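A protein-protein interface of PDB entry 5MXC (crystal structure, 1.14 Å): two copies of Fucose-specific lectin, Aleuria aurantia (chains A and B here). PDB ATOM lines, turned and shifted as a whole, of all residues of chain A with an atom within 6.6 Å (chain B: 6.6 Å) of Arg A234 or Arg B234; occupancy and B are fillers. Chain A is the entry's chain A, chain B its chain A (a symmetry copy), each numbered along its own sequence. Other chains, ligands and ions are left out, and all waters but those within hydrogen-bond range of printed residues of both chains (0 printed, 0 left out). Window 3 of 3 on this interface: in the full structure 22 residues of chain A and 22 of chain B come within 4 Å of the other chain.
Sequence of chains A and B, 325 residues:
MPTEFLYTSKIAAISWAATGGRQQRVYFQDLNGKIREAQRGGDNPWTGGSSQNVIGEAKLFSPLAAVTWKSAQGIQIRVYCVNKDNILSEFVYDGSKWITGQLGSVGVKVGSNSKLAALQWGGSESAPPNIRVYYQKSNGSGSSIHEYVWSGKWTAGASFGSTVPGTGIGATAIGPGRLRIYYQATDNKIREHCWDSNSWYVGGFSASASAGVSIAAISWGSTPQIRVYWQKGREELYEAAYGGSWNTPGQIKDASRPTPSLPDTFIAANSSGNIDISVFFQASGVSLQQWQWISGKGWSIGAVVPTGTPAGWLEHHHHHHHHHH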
ATOM      1  N   GLN A 231      14.784  -7.972 -30.251  1.00  0.00           N
ATOM      2  CA  GLN A 231      15.770  -7.188 -29.519  1.00  0.00           C
ATOM      3  C   GLN A 231      15.112  -6.483 -28.362  1.00  0.00           C
ATOM      4  O   GLN A 231      14.075  -5.815 -28.531  1.00  0.00           O
ATOM      5  CB  GLN A 231      16.416  -6.152 -30.444  1.00  0.00           C
ATOM      6  CG  GLN A 231      17.572  -5.366 -29.839  1.00  0.00           C
ATOM      7  CD  GLN A 231      18.043  -4.294 -30.788  1.00  0.00           C
ATOM      8  OE1 GLN A 231      18.846  -4.555 -31.689  1.00  0.00           O
ATOM      9  NE2 GLN A 231      17.505  -3.093 -30.631  1.00  0.00           N
ATOM     10  N   LYS A 232      15.730  -6.615 -27.188  1.00  0.00           N
ATOM     11  CA  LYS A 232      15.427  -5.746 -26.055  1.00  0.00           C
ATOM     12  C   LYS A 232      16.415  -4.587 -26.097  1.00  0.00           C
ATOM     13  O   LYS A 232      17.605  -4.780 -26.377  1.00  0.00           O
ATOM     14  CB  LYS A 232      15.542  -6.511 -24.733  1.00  0.00           C
ATOM     15  CG  LYS A 232      15.531  -5.633 -23.490  1.00  0.00           C
ATOM     16  CD  LYS A 232      15.209  -6.429 -22.231  1.00  0.00           C
ATOM     17  CE  LYS A 232      15.267  -5.541 -20.995  1.00  0.00           C
ATOM     18  NZ  LYS A 232      15.404  -6.353 -19.760  1.00  0.00           N
ATOM     19  N   GLY A 233      15.941  -3.372 -25.810  1.00  0.00           N
ATOM     20  CA  GLY A 233      16.837  -2.224 -25.882  1.00  0.00           C
ATOM     21  C   GLY A 233      18.053  -2.399 -24.989  1.00  0.00           C
ATOM     22  O   GLY A 233      17.939  -2.868 -23.850  1.00  0.00           O
ATOM     23  N   ARG A 234      19.213  -2.041 -25.536  1.00  0.00           N
ATOM     24  CA  ARG A 234      20.528  -2.211 -24.890  1.00  0.00           C
ATOM     25  C   ARG A 234      20.885  -3.680 -24.630  1.00  0.00           C
ATOM     26  O   ARG A 234      21.684  -4.003 -23.740  1.00  0.00           O
ATOM     27  CB  ARG A 234      20.695  -1.330 -23.642  1.00  0.00           C
ATOM     28  CG  ARG A 234      22.148  -0.893 -23.426  1.00  0.00           C
ATOM     29  CD  ARG A 234      22.257  -0.070 -22.158  1.00  0.00           C
ATOM     30  NE  ARG A 234      23.563   0.557 -22.008  1.00  0.00           N
ATOM     31  CZ  ARG A 234      24.663  -0.047 -21.551  1.00  0.00           C
ATOM     32  NH1 ARG A 234      24.655  -1.330 -21.183  1.00  0.00           N
ATOM     33  NH2 ARG A 234      25.797   0.651 -21.455  1.00  0.00           N
ATOM     34  N   GLU A 235      20.311  -4.564 -25.446  1.00  0.00           N
ATOM     35  CA  GLU A 235      20.783  -5.941 -25.570  1.00  0.00           C
ATOM     36  C   GLU A 235      21.042  -6.195 -27.044  1.00  0.00           C
ATOM     37  O   GLU A 235      20.625  -5.413 -27.916  1.00  0.00           O
ATOM     38  CB  GLU A 235      19.751  -6.935 -25.049  1.00  0.00           C
ATOM     39  CG  GLU A 235      19.346  -6.723 -23.603  1.00  0.00           C
ATOM     40  CD  GLU A 235      20.475  -6.908 -22.599  1.00  0.00           C
ATOM     41  OE1 GLU A 235      20.297  -6.413 -21.469  1.00  0.00           O
ATOM     42  OE2 GLU A 235      21.507  -7.534 -22.917  1.00  0.00           O
ATOM     43  N   GLU A 236      21.723  -7.286 -27.369  1.00  0.00           N
ATOM     44  CA  GLU A 236      22.024  -7.543 -28.773  1.00  0.00           C
ATOM     45  C   GLU A 236      20.787  -8.049 -29.529  1.00  0.00           C
ATOM     46  O   GLU A 236      19.883  -8.667 -28.951  1.00  0.00           O
ATOM     47  CB  GLU A 236      23.163  -8.558 -28.936  1.00  0.00           C
ATOM     48  CG  GLU A 236      24.470  -8.236 -28.211  1.00  0.00           C
ATOM     49  CD  GLU A 236      25.239  -7.034 -28.736  1.00  0.00           C
ATOM     50  OE1 GLU A 236      24.819  -6.317 -29.666  1.00  0.00           O
ATOM     51  OE2 GLU A 236      26.346  -6.779 -28.192  1.00  0.00           O
ATOM     52  N   PRO A 258      29.289  -2.904 -28.713  1.00  0.00           N
ATOM     53  CA  PRO A 258      28.340  -3.758 -28.012  1.00  0.00           C
ATOM     54  C   PRO A 258      27.005  -3.073 -27.740  1.00  0.00           C
ATOM     55  O   PRO A 258      26.941  -1.854 -27.530  1.00  0.00           O
ATOM     56  CB  PRO A 258      29.057  -4.087 -26.697  1.00  0.00           C
ATOM     57  CG  PRO A 258      29.994  -2.947 -26.505  1.00  0.00           C
ATOM     58  CD  PRO A 258      30.473  -2.604 -27.881  1.00  0.00           C
ATOM     59  N   THR A 259      25.952  -3.890 -27.778  1.00  0.00           N
ATOM     60  CA  THR A 259      24.580  -3.507 -27.427  1.00  0.00           C
ATOM     61  C   THR A 259      24.264  -2.055 -27.790  1.00  0.00           C
ATOM     62  O   THR A 259      24.004  -1.243 -26.916  1.00  0.00           O
ATOM     63  CB  THR A 259      24.298  -3.773 -25.931  1.00  0.00           C
ATOM     64  OG1 THR A 259      25.145  -2.967 -25.102  1.00  0.00           O
ATOM     65  CG2 THR A 259      24.514  -5.241 -25.570  1.00  0.00           C
ATOM     66  N   PRO A 260      24.292  -1.727 -29.092  1.00  0.00           N
ATOM     67  CA  PRO A 260      24.313  -0.330 -29.514  1.00  0.00           C
ATOM     68  C   PRO A 260      23.003   0.445 -29.380  1.00  0.00           C
ATOM     69  O   PRO A 260      23.028   1.657 -29.566  1.00  0.00           O
ATOM     70  CB  PRO A 260      24.756  -0.419 -30.978  1.00  0.00           C
ATOM     71  CG  PRO A 260      24.267  -1.738 -31.426  1.00  0.00           C
ATOM     72  CD  PRO A 260      24.493  -2.629 -30.240  1.00  0.00           C
ATOM     73  N   SER A 261      21.887  -0.213 -29.079  1.00  0.00           N
ATOM     74  CA  SER A 261      20.611   0.478 -28.922  1.00  0.00           C
ATOM     75  C   SER A 261      20.448   1.010 -27.512  1.00  0.00           C
ATOM     76  O   SER A 261      21.087   0.522 -26.574  1.00  0.00           O
ATOM     77  CB  SER A 261      19.450  -0.464 -29.259  1.00  0.00           C
ATOM     78  OG  SER A 261      19.355  -1.552 -28.352  1.00  0.00           O
ATOM     79  N   LEU A 262      19.572   2.004 -27.368  1.00  0.00           N
ATOM     80  CA  LEU A 262      19.222   2.528 -26.059  1.00  0.00           C
ATOM     81  C   LEU A 262      18.191   1.627 -25.360  1.00  0.00           C
ATOM     82  O   LEU A 262      17.438   0.875 -26.012  1.00  0.00           O
ATOM     83  CB  LEU A 262      18.659   3.944 -26.164  1.00  0.00           C
ATOM     84  CG  LEU A 262      19.673   5.022 -26.549  1.00  0.00           C
ATOM     85  CD1 LEU A 262      18.929   6.281 -26.937  1.00  0.00           C
ATOM     86  CD2 LEU A 262      20.653   5.289 -25.408  1.00  0.00           C
ATOM     87  N   PRO A 263      18.095   1.724 -24.026  1.00  0.00           N
ATOM     88  CA  PRO A 263      17.051   0.989 -23.317  1.00  0.00           C
ATOM     89  C   PRO A 263      15.639   1.303 -23.824  1.00  0.00           C
ATOM     90  O   PRO A 263      15.365   2.435 -24.233  1.00  0.00           O
ATOM     91  CB  PRO A 263      17.232   1.464 -21.871  1.00  0.00           C
ATOM     92  CG  PRO A 263      18.668   1.851 -21.777  1.00  0.00           C
ATOM     93  CD  PRO A 263      18.965   2.470 -23.094  1.00  0.00           C
ATOM     94  N   ASP A 264      14.779   0.281 -23.817  1.00  0.00           N
ATOM     95  CA  ASP A 264      13.335   0.415 -24.039  1.00  0.00           C
ATOM     96  C   ASP A 264      12.955   0.886 -25.447  1.00  0.00           C
ATOM     97  O   ASP A 264      11.848   1.355 -25.677  1.00  0.00           O
ATOM     98  CB  ASP A 264      12.723   1.279 -22.933  1.00  0.00           C
ATOM     99  CG  ASP A 264      13.181   0.824 -21.570  1.00  0.00           C
ATOM    100  OD1 ASP A 264      13.024  -0.376 -21.281  1.00  0.00           O
ATOM    101  OD2 ASP A 264      13.769   1.637 -20.839  1.00  0.00           O
ATOM    102  N   THR A 265      13.851   0.674 -26.409  1.00  0.00           N
ATOM    103  CA  THR A 265      13.645   1.079 -27.787  1.00  0.00           C
ATOM    104  C   THR A 265      13.161  -0.098 -28.649  1.00  0.00           C
ATOM    105  O   THR A 265      13.117  -1.251 -28.205  1.00  0.00           O
ATOM    106  CB  THR A 265      14.953   1.646 -28.373  1.00  0.00           C
ATOM    107  OG1 THR A 265      15.977   0.657 -28.272  1.00  0.00           O
ATOM    108  CG2 THR A 265      15.374   2.921 -27.665  1.00  0.00           C
ATOM    109  N   GLN B 231      27.632  12.799 -12.271  1.00  0.00           N
ATOM    110  CA  GLN B 231      27.064  11.553 -12.767  1.00  0.00           C
ATOM    111  C   GLN B 231      27.105  11.530 -14.272  1.00  0.00           C
ATOM    112  O   GLN B 231      26.672  12.492 -14.935  1.00  0.00           O
ATOM    113  CB  GLN B 231      25.613  11.408 -12.297  1.00  0.00           C
ATOM    114  CG  GLN B 231      24.949  10.076 -12.623  1.00  0.00           C
ATOM    115  CD  GLN B 231      23.494  10.094 -12.231  1.00  0.00           C
ATOM    116  OE1 GLN B 231      23.149   9.849 -11.071  1.00  0.00           O
ATOM    117  NE2 GLN B 231      22.635  10.442 -13.178  1.00  0.00           N
ATOM    118  N   LYS B 232      27.608  10.420 -14.812  1.00  0.00           N
ATOM    119  CA  LYS B 232      27.420  10.095 -16.223  1.00  0.00           C
ATOM    120  C   LYS B 232      26.181   9.214 -16.323  1.00  0.00           C
ATOM    121  O   LYS B 232      25.969   8.324 -15.490  1.00  0.00           O
ATOM    122  CB  LYS B 232      28.649   9.372 -16.786  1.00  0.00           C
ATOM    123  CG  LYS B 232      28.439   8.739 -18.153  1.00  0.00           C
ATOM    124  CD  LYS B 232      29.759   8.428 -18.847  1.00  0.00           C
ATOM    125  CE  LYS B 232      29.522   7.738 -20.185  1.00  0.00           C
ATOM    126  NZ  LYS B 232      30.748   7.040 -20.649  1.00  0.00           N
ATOM    127  N   GLY B 233      25.354   9.442 -17.346  1.00  0.00           N
ATOM    128  CA  GLY B 233      24.130   8.656 -17.459  1.00  0.00           C
ATOM    129  C   GLY B 233      24.418   7.165 -17.502  1.00  0.00           C
ATOM    130  O   GLY B 233      25.355   6.721 -18.176  1.00  0.00           O
ATOM    131  N   ARG B 234      23.614   6.412 -16.753  1.00  0.00           N
ATOM    132  CA  ARG B 234      23.766   4.957 -16.570  1.00  0.00           C
ATOM    133  C   ARG B 234      25.082   4.572 -15.884  1.00  0.00           C
ATOM    134  O   ARG B 234      25.587   3.450 -16.037  1.00  0.00           O
ATOM    135  CB  ARG B 234      23.518   4.166 -17.864  1.00  0.00           C
ATOM    136  CG  ARG B 234      22.922   2.780 -17.596  1.00  0.00           C
ATOM    137  CD  ARG B 234      22.744   2.032 -18.902  1.00  0.00           C
ATOM    138  NE  ARG B 234      21.986   0.799 -18.743  1.00  0.00           N
ATOM    139  CZ  ARG B 234      22.477  -0.361 -18.300  1.00  0.00           C
ATOM    140  NH1 ARG B 234      23.758  -0.489 -17.948  1.00  0.00           N
ATOM    141  NH2 ARG B 234      21.669  -1.419 -18.212  1.00  0.00           N
ATOM    142  N   GLU B 235      25.612   5.504 -15.093  1.00  0.00           N
ATOM    143  CA  GLU B 235      26.654   5.204 -14.113  1.00  0.00           C
ATOM    144  C   GLU B 235      26.165   5.713 -12.768  1.00  0.00           C
ATOM    145  O   GLU B 235      25.188   6.476 -12.685  1.00  0.00           O
ATOM    146  CB  GLU B 235      27.972   5.881 -14.472  1.00  0.00           C
ATOM    147  CG  GLU B 235      28.517   5.515 -15.839  1.00  0.00           C
ATOM    148  CD  GLU B 235      28.881   4.046 -16.000  1.00  0.00           C
ATOM    149  OE1 GLU B 235      28.989   3.627 -17.168  1.00  0.00           O
ATOM    150  OE2 GLU B 235      29.062   3.326 -14.995  1.00  0.00           O
ATOM    151  N   GLU B 236      26.824   5.319 -11.686  1.00  0.00           N
ATOM    152  CA  GLU B 236      26.359   5.758 -10.376  1.00  0.00           C
ATOM    153  C   GLU B 236      26.730   7.223 -10.109  1.00  0.00           C
ATOM    154  O   GLU B 236      27.718   7.748 -10.639  1.00  0.00           O
ATOM    155  CB  GLU B 236      26.925   4.884  -9.247  1.00  0.00           C
ATOM    156  CG  GLU B 236      26.686   3.378  -9.369  1.00  0.00           C
ATOM    157  CD  GLU B 236      25.242   2.925  -9.226  1.00  0.00           C
ATOM    158  OE1 GLU B 236      24.296   3.721  -9.069  1.00  0.00           O
ATOM    159  OE2 GLU B 236      25.024   1.684  -9.267  1.00  0.00           O
ATOM    160  N   PRO B 258      20.789  -0.759  -9.476  1.00  0.00           N
ATOM    161  CA  PRO B 258      22.047  -0.248 -10.003  1.00  0.00           C
ATOM    162  C   PRO B 258      21.859   0.755 -11.136  1.00  0.00           C
ATOM    163  O   PRO B 258      20.905   0.664 -11.921  1.00  0.00           O
ATOM    164  CB  PRO B 258      22.763  -1.507 -10.507  1.00  0.00           C
ATOM    165  CG  PRO B 258      21.655  -2.457 -10.797  1.00  0.00           C
ATOM    166  CD  PRO B 258      20.643  -2.210  -9.722  1.00  0.00           C
ATOM    167  N   THR B 259      22.779   1.719 -11.173  1.00  0.00           N
ATOM    168  CA  THR B 259      22.897   2.726 -12.233  1.00  0.00           C
ATOM    169  C   THR B 259      21.540   3.128 -12.816  1.00  0.00           C
ATOM    170  O   THR B 259      21.277   2.894 -13.985  1.00  0.00           O
ATOM    171  CB  THR B 259      23.853   2.245 -13.349  1.00  0.00           C
ATOM    172  OG1 THR B 259      23.337   1.072 -13.990  1.00  0.00           O
ATOM    173  CG2 THR B 259      25.244   1.933 -12.801  1.00  0.00           C
ATOM    174  N   PRO B 260      20.671   3.732 -11.990  1.00  0.00           N
ATOM    175  CA  PRO B 260      19.264   3.871 -12.352  1.00  0.00           C
ATOM    176  C   PRO B 260      18.930   4.916 -13.415  1.00  0.00           C
ATOM    177  O   PRO B 260      17.788   4.943 -13.860  1.00  0.00           O
ATOM    178  CB  PRO B 260      18.596   4.209 -11.015  1.00  0.00           C
ATOM    179  CG  PRO B 260      19.650   4.902 -10.248  1.00  0.00           C
ATOM    180  CD  PRO B 260      20.903   4.155 -10.597  1.00  0.00           C
ATOM    181  N   SER B 261      19.877   5.763 -13.812  1.00  0.00           N
ATOM    182  CA  SER B 261      19.619   6.770 -14.836  1.00  0.00           C
ATOM    183  C   SER B 261      19.818   6.200 -16.226  1.00  0.00           C
ATOM    184  O   SER B 261      20.521   5.200 -16.405  1.00  0.00           O
ATOM    185  CB  SER B 261      20.538   7.981 -14.635  1.00  0.00           C
ATOM    186  OG  SER B 261      21.908   7.656 -14.822  1.00  0.00           O
ATOM    187  N   LEU B 262      19.205   6.856 -17.211  1.00  0.00           N
ATOM    188  CA  LEU B 262      19.406   6.497 -18.605  1.00  0.00           C
ATOM    189  C   LEU B 262      20.721   7.082 -19.143  1.00  0.00           C
ATOM    190  O   LEU B 262      21.248   8.086 -18.619  1.00  0.00           O
ATOM    191  CB  LEU B 262      18.248   6.987 -19.472  1.00  0.00           C
ATOM    192  CG  LEU B 262      16.921   6.256 -19.265  1.00  0.00           C
ATOM    193  CD1 LEU B 262      15.814   7.048 -19.923  1.00  0.00           C
ATOM    194  CD2 LEU B 262      16.985   4.832 -19.816  1.00  0.00           C
ATOM    195  N   PRO B 263      21.249   6.506 -20.233  1.00  0.00           N
ATOM    196  CA  PRO B 263      22.428   7.093 -20.866  1.00  0.00           C
ATOM    197  C   PRO B 263      22.234   8.559 -21.267  1.00  0.00           C
ATOM    198  O   PRO B 263      21.126   8.957 -21.639  1.00  0.00           O
ATOM    199  CB  PRO B 263      22.618   6.207 -22.102  1.00  0.00           C
ATOM    200  CG  PRO B 263      22.014   4.897 -21.725  1.00  0.00           C
ATOM    201  CD  PRO B 263      20.827   5.264 -20.911  1.00  0.00           C
ATOM    202  N   ASP B 264      23.310   9.340 -21.152  1.00  0.00           N
ATOM    203  CA  ASP B 264      23.406  10.701 -21.692  1.00  0.00           C
ATOM    204  C   ASP B 264      22.453  11.707 -21.038  1.00  0.00           C
ATOM    205  O   ASP B 264      22.180  12.766 -21.587  1.00  0.00           O
ATOM    206  CB  ASP B 264      23.276  10.658 -23.217  1.00  0.00           C
ATOM    207  CG  ASP B 264      24.178   9.605 -23.811  1.00  0.00           C
ATOM    208  OD1 ASP B 264      25.385   9.643 -23.507  1.00  0.00           O
ATOM    209  OD2 ASP B 264      23.669   8.705 -24.497  1.00  0.00           O
ATOM    210  N   THR B 265      22.018  11.408 -19.815  1.00  0.00           N
ATOM    211  CA  THR B 265      21.097  12.251 -19.074  1.00  0.00           C
ATOM    212  C   THR B 265      21.843  13.138 -18.064  1.00  0.00           C
ATOM    213  O   THR B 265      23.053  13.000 -17.849  1.00  0.00           O
ATOM    214  CB  THR B 265      20.062  11.381 -18.333  1.00  0.00           C
ATOM    215  OG1 THR B 265      20.748  10.476 -17.468  1.00  0.00           O
ATOM    216  CG2 THR B 265      19.178  10.620 -19.304  1.00  0.00           C
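Among the printed residues, merely in contact across the chains: Pro A263 with Leu B262 and Leu A262 with Pro B263.
Lys A232 touches none of the printed residues of chain B.
Of the printed residues of chain B, Arg A234 touches Arg B234.
Pro A260 touches none of the printed residues of chain B.
Of the printed residues of chain B, Leu A262 touches Pro B263 (3.9 Å).
Of the printed residues of chain B, Pro A263 touches Leu B262.
Printed residues of chain A within 4 Å of Leu B262: Pro A263.
Of the printed residues of chain A, Pro B263 touches Leu A262 (3.9 Å).
The nearest printed residue of chain B that does not touch Arg A234 is Pro B263 (4.6 Å).
The nearest printed residue of chain A that does not touch Arg B234 is Pro A263 (4.6 Å).
The nearest printed residue of chain B that does not touch Pro A263 is Pro B263 (4.005 Å).
Of the 14 printed residues of chain B, 3 touch a printed residue of chain A.
Hydrophobic or aromatic side chains of chain B that line the printed part of chain A: Leu B262 and Pro B263.
Hydrophobic or aromatic side chains of chain A within 4 Å of the printed part of chain B: Leu A262 and Pro A263.
Among the printed residues, 3 pairs touch across the chains.
Among the printed residues, no Asp or Glu carboxylate lies within 4 Å of a Lys or Arg side-chain nitrogen of the other chain.
Arg B234 touches its own counterpart, Arg A234.
Leu A262 touches Pro B263, and with the chains exchanged Pro A263 touches Leu B262.
Positions printed for both chains: 231, 232, 233, 234, 235, 236, 258, 259, 260, 261, 262, 263, 264 and 265.
Of the 3 pairs that touch across the chains among the printed residues, 3 have their exchanged pair printed and touching as well.
The side-chain hydroxyl (OG) of Ser A261 lies within hydrogen-bond range of the backbone NH (N) of Arg A234, at 2.9 Å.
The backbone NH (N) of Arg A234 lies within hydrogen-bond range of the backbone carbonyl oxygen (O) of Leu A262 (3.4 Å).
The backbone carbonyl oxygen (O) of Leu A262 is in hydrogen-bond range of the side-chain hydroxyl (OG1) of Thr A265, 2.7 Å away.
The backbone NH (N) of Arg B234 lies within hydrogen-bond range of the side-chain hydroxyl (OG) of Ser B261.
N of Arg B234 sits at hydrogen-bond distance from O of Leu B262 (3.4 Å).
The side-chain hydroxyl of Thr B265 lies within hydrogen-bond range of the backbone carbonyl oxygen of Leu B262, 2.7 Å away.
The guanidinium group of Arg B234 sits close to the guanidinium group of Arg A234, 3.5 Å away.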
